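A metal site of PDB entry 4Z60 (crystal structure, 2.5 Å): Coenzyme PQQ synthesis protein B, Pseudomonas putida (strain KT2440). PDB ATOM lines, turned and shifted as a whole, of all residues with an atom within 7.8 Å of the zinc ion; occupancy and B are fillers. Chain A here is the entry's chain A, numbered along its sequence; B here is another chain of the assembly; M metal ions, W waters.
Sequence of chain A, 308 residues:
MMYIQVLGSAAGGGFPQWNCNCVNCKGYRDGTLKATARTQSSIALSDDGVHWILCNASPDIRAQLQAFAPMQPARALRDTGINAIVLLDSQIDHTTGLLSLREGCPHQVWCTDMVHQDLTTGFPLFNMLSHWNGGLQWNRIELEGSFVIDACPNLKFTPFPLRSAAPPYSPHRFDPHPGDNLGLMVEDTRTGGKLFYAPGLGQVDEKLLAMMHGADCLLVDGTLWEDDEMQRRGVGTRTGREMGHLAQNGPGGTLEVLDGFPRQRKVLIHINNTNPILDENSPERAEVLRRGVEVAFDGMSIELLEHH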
ATOM      1  N   ALA A  10       7.854   2.838 -25.307  1.00  0.00           N
ATOM      2  CA  ALA A  10       7.342   2.636 -26.656  1.00  0.00           C
ATOM      3  C   ALA A  10       6.797   1.225 -26.817  1.00  0.00           C
ATOM      4  O   ALA A  10       7.125   0.329 -26.054  1.00  0.00           O
ATOM      5  CB  ALA A  10       8.443   2.899 -27.706  1.00  0.00           C
ATOM      6  N   ALA A  11       5.949   1.044 -27.830  1.00  0.00           N
ATOM      7  CA  ALA A  11       5.513  -0.292 -28.228  1.00  0.00           C
ATOM      8  C   ALA A  11       6.675  -1.003 -28.917  1.00  0.00           C
ATOM      9  O   ALA A  11       7.769  -0.437 -29.026  1.00  0.00           O
ATOM     10  CB  ALA A  11       4.313  -0.195 -29.149  1.00  0.00           C
ATOM     11  N   GLY A  12       6.459  -2.230 -29.380  1.00  0.00           N
ATOM     12  CA  GLY A  12       7.484  -2.960 -30.103  1.00  0.00           C
ATOM     13  C   GLY A  12       8.039  -2.161 -31.269  1.00  0.00           C
ATOM     14  O   GLY A  12       7.298  -1.461 -31.967  1.00  0.00           O
ATOM     15  N   GLY A  13       9.344  -2.246 -31.472  1.00  0.00           N
ATOM     16  CA  GLY A  13       9.999  -1.500 -32.538  1.00  0.00           C
ATOM     17  C   GLY A  13      10.638  -0.215 -32.042  1.00  0.00           C
ATOM     18  O   GLY A  13      11.539   0.325 -32.673  1.00  0.00           O
ATOM     19  N   GLN A  40      11.772   0.186 -26.034  1.00  0.00           N
ATOM     20  CA  GLN A  40      10.636  -0.725 -25.906  1.00  0.00           C
ATOM     21  C   GLN A  40      10.216  -0.964 -24.457  1.00  0.00           C
ATOM     22  O   GLN A  40      11.057  -1.056 -23.561  1.00  0.00           O
ATOM     23  CB  GLN A  40      10.895  -2.031 -26.657  1.00  0.00           C
ATOM     24  CG  GLN A  40      10.615  -1.892 -28.143  1.00  0.00           C
ATOM     25  CD  GLN A  40      11.404  -2.861 -28.992  1.00  0.00           C
ATOM     26  OE1 GLN A  40      10.858  -3.831 -29.508  1.00  0.00           O
ATOM     27  NE2 GLN A  40      12.700  -2.596 -29.141  1.00  0.00           N
ATOM     28  N   SER A  41       8.903  -1.083 -24.250  1.00  0.00           N
ATOM     29  CA  SER A  41       8.274  -1.052 -22.935  1.00  0.00           C
ATOM     30  C   SER A  41       8.871  -1.957 -21.861  1.00  0.00           C
ATOM     31  O   SER A  41       8.994  -3.165 -22.043  1.00  0.00           O
ATOM     32  CB  SER A  41       6.779  -1.317 -23.051  1.00  0.00           C
ATOM     33  OG  SER A  41       6.078  -0.091 -23.156  1.00  0.00           O
ATOM     34  N   ASN A  56       9.007  -7.259 -17.650  1.00  0.00           N
ATOM     35  CA  ASN A  56       9.399  -7.438 -19.046  1.00  0.00           C
ATOM     36  C   ASN A  56      10.841  -7.040 -19.298  1.00  0.00           C
ATOM     37  O   ASN A  56      11.297  -6.005 -18.828  1.00  0.00           O
ATOM     38  CB  ASN A  56       8.448  -6.720 -20.015  1.00  0.00           C
ATOM     39  CG  ASN A  56       7.031  -7.280 -19.973  1.00  0.00           C
ATOM     40  OD1 ASN A  56       6.810  -8.400 -19.518  1.00  0.00           O
ATOM     41  ND2 ASN A  56       6.074  -6.492 -20.442  1.00  0.00           N
ATOM     42  N   ASP A  89       3.882 -11.650 -20.616  1.00  0.00           N
ATOM     43  CA  ASP A  89       3.598 -12.519 -21.741  1.00  0.00           C
ATOM     44  C   ASP A  89       4.903 -13.070 -22.294  1.00  0.00           C
ATOM     45  O   ASP A  89       5.971 -12.750 -21.789  1.00  0.00           O
ATOM     46  CB  ASP A  89       2.821 -11.770 -22.828  1.00  0.00           C
ATOM     47  CG  ASP A  89       3.480 -10.454 -23.193  1.00  0.00           C
ATOM     48  OD1 ASP A  89       4.612 -10.489 -23.718  1.00  0.00           O
ATOM     49  OD2 ASP A  89       2.869  -9.389 -22.978  1.00  0.00           O
ATOM     50  N   GLN A  91       5.931 -12.662 -25.458  1.00  0.00           N
ATOM     51  CA  GLN A  91       6.265 -11.965 -26.694  1.00  0.00           C
ATOM     52  C   GLN A  91       7.746 -11.603 -26.773  1.00  0.00           C
ATOM     53  O   GLN A  91       8.400 -11.391 -25.747  1.00  0.00           O
ATOM     54  CB  GLN A  91       5.387 -10.729 -26.855  1.00  0.00           C
ATOM     55  CG  GLN A  91       3.927 -11.047 -27.057  1.00  0.00           C
ATOM     56  CD  GLN A  91       3.049  -9.816 -26.954  1.00  0.00           C
ATOM     57  OE1 GLN A  91       3.535  -8.686 -26.982  1.00  0.00           O
ATOM     58  NE2 GLN A  91       1.738 -10.030 -26.835  1.00  0.00           N
ATOM     59  N   ILE A  92       8.253 -11.536 -27.990  1.00  0.00           N
ATOM     60  CA  ILE A  92       9.674 -11.308 -28.256  1.00  0.00           C
ATOM     61  C   ILE A  92      10.187  -9.981 -27.689  1.00  0.00           C
ATOM     62  O   ILE A  92      11.275  -9.923 -27.127  1.00  0.00           O
ATOM     63  CB  ILE A  92       9.952 -11.400 -29.769  1.00  0.00           C
ATOM     64  CG1 ILE A  92       9.785 -12.838 -30.249  1.00  0.00           C
ATOM     65  CG2 ILE A  92      11.351 -10.894 -30.104  1.00  0.00           C
ATOM     66  CD1 ILE A  92      10.094 -13.025 -31.711  1.00  0.00           C
ATOM     67  N   ASP A  93       9.407  -8.914 -27.833  1.00  0.00           N
ATOM     68  CA  ASP A  93       9.833  -7.608 -27.333  1.00  0.00           C
ATOM     69  C   ASP A  93       9.768  -7.496 -25.798  1.00  0.00           C
ATOM     70  O   ASP A  93      10.199  -6.485 -25.232  1.00  0.00           O
ATOM     71  CB  ASP A  93       9.052  -6.472 -28.006  1.00  0.00           C
ATOM     72  CG  ASP A  93       7.551  -6.695 -28.021  1.00  0.00           C
ATOM     73  OD1 ASP A  93       7.124  -7.869 -27.928  1.00  0.00           O
ATOM     74  OD2 ASP A  93       6.797  -5.710 -28.148  1.00  0.00           O
ATOM     75  N   HIS A  94       9.266  -8.524 -25.128  1.00  0.00           N
ATOM     76  CA  HIS A  94       9.163  -8.504 -23.668  1.00  0.00           C
ATOM     77  C   HIS A  94      10.055  -9.531 -22.984  1.00  0.00           C
ATOM     78  O   HIS A  94      10.082  -9.603 -21.761  1.00  0.00           O
ATOM     79  CB  HIS A  94       7.709  -8.718 -23.231  1.00  0.00           C
ATOM     80  CG  HIS A  94       6.749  -7.748 -23.824  1.00  0.00           C
ATOM     81  ND1 HIS A  94       5.414  -8.018 -23.963  1.00  0.00           N
ATOM     82  CD2 HIS A  94       6.935  -6.497 -24.312  1.00  0.00           C
ATOM     83  CE1 HIS A  94       4.809  -6.978 -24.526  1.00  0.00           C
ATOM     84  NE2 HIS A  94       5.716  -6.039 -24.747  1.00  0.00           N
ATOM     85  N   PRO A 199      -0.035  -2.704 -19.784  1.00  0.00           N
ATOM     86  CA  PRO A 199       0.568  -2.170 -21.012  1.00  0.00           C
ATOM     87  C   PRO A 199      -0.132  -2.692 -22.256  1.00  0.00           C
ATOM     88  O   PRO A 199      -0.194  -2.005 -23.278  1.00  0.00           O
ATOM     89  CB  PRO A 199       2.001  -2.700 -20.946  1.00  0.00           C
ATOM     90  CG  PRO A 199       1.889  -3.972 -20.161  1.00  0.00           C
ATOM     91  CD  PRO A 199       0.811  -3.721 -19.147  1.00  0.00           C
ATOM     92  N   GLY A 200      -0.659  -3.905 -22.163  1.00  0.00           N
ATOM     93  CA  GLY A 200      -1.364  -4.529 -23.268  1.00  0.00           C
ATOM     94  C   GLY A 200      -2.814  -4.767 -22.902  1.00  0.00           C
ATOM     95  O   GLY A 200      -3.148  -5.739 -22.221  1.00  0.00           O
ATOM     96  N   THR A 223      -0.885   2.359 -27.127  1.00  0.00           N
ATOM     97  CA  THR A 223      -0.235   2.037 -28.392  1.00  0.00           C
ATOM     98  C   THR A 223      -0.707   2.896 -29.560  1.00  0.00           C
ATOM     99  O   THR A 223       0.100   3.581 -30.209  1.00  0.00           O
ATOM    100  CB  THR A 223      -0.440   0.554 -28.751  1.00  0.00           C
ATOM    101  OG1 THR A 223      -0.122  -0.260 -27.610  1.00  0.00           O
ATOM    102  CG2 THR A 223       0.455   0.163 -29.919  1.00  0.00           C
ATOM    103  N   HIS A 245      -4.896  -4.193 -28.921  1.00  0.00           N
ATOM    104  CA  HIS A 245      -4.703  -2.877 -28.322  1.00  0.00           C
ATOM    105  C   HIS A 245      -5.939  -2.011 -28.524  1.00  0.00           C
ATOM    106  O   HIS A 245      -6.435  -1.851 -29.644  1.00  0.00           O
ATOM    107  CB  HIS A 245      -3.480  -2.179 -28.912  1.00  0.00           C
ATOM    108  CG  HIS A 245      -2.195  -2.939 -28.725  1.00  0.00           C
ATOM    109  ND1 HIS A 245      -1.722  -3.298 -27.480  1.00  0.00           N
ATOM    110  CD2 HIS A 245      -1.299  -3.395 -29.627  1.00  0.00           C
ATOM    111  CE1 HIS A 245      -0.578  -3.949 -27.624  1.00  0.00           C
ATOM    112  NE2 HIS A 245      -0.304  -4.025 -28.915  1.00  0.00           N
ATOM    113  N   HIS A 270       3.589   2.188 -23.537  1.00  0.00           N
ATOM    114  CA  HIS A 270       3.663   1.235 -24.647  1.00  0.00           C
ATOM    115  C   HIS A 270       3.095   1.894 -25.912  1.00  0.00           C
ATOM    116  O   HIS A 270       2.184   1.389 -26.544  1.00  0.00           O
ATOM    117  CB  HIS A 270       2.922  -0.064 -24.294  1.00  0.00           C
ATOM    118  CG  HIS A 270       3.081  -1.163 -25.294  1.00  0.00           C
ATOM    119  ND1 HIS A 270       2.234  -1.330 -26.376  1.00  0.00           N
ATOM    120  CD2 HIS A 270       3.980  -2.182 -25.357  1.00  0.00           C
ATOM    121  CE1 HIS A 270       2.613  -2.387 -27.071  1.00  0.00           C
ATOM    122  NE2 HIS A 270       3.669  -2.919 -26.479  1.00  0.00           N
ATOM    123  N   ARG B 102      12.448  -8.171 -37.041  1.00  0.00           N
ATOM    124  CA  ARG B 102      11.273  -8.950 -37.449  1.00  0.00           C
ATOM    125  C   ARG B 102      10.248  -8.140 -38.248  1.00  0.00           C
ATOM    126  O   ARG B 102       9.511  -8.690 -39.055  1.00  0.00           O
ATOM    127  CB  ARG B 102      10.616  -9.637 -36.239  1.00  0.00           C
ATOM    128  CG  ARG B 102      10.120  -8.699 -35.153  1.00  0.00           C
ATOM    129  CD  ARG B 102       9.975  -9.400 -33.801  1.00  0.00           C
ATOM    130  NE  ARG B 102       9.495  -8.498 -32.756  1.00  0.00           N
ATOM    131  CZ  ARG B 102      10.234  -7.544 -32.177  1.00  0.00           C
ATOM    132  NH1 ARG B 102       9.702  -6.772 -31.241  1.00  0.00           N
ATOM    133  NH2 ARG B 102      11.499  -7.366 -32.540  1.00  0.00           N
HETATM  134 ZN    ZN M   1       5.290  -4.605 -26.710  1.00  0.00          ZN
HETATM  135  O   HOH W   1       7.332  -3.391 -25.875  1.00  0.00           O
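The zinc ion is bound by a ring nitrogen (NE2) of His 270 (2.4 Å), the side-chain carboxylate (OD2) of Asp 93 (2.4 Å), a ring nitrogen (NE2) of His 94 (2.5 Å) and water W1 (2.5 Å). The zinc ion has four donor atoms within binding distance.
N of His 270 sits close to OG of Ser 41. A ring nitrogen (ND1) of His 270 is in hydrogen-bond range of the side-chain hydroxyl (OG1) of Thr 223. A ring nitrogen (ND1) of His 94 sits at hydrogen-bond distance from the side-chain carboxylate (OD1) of Asp 89, at 2.6 Å.
Residues that only touch the zinc ion: Gly 12 (3.8 Å). Of the 18 residues printed, 4 come within 4 Å of the zinc ion.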
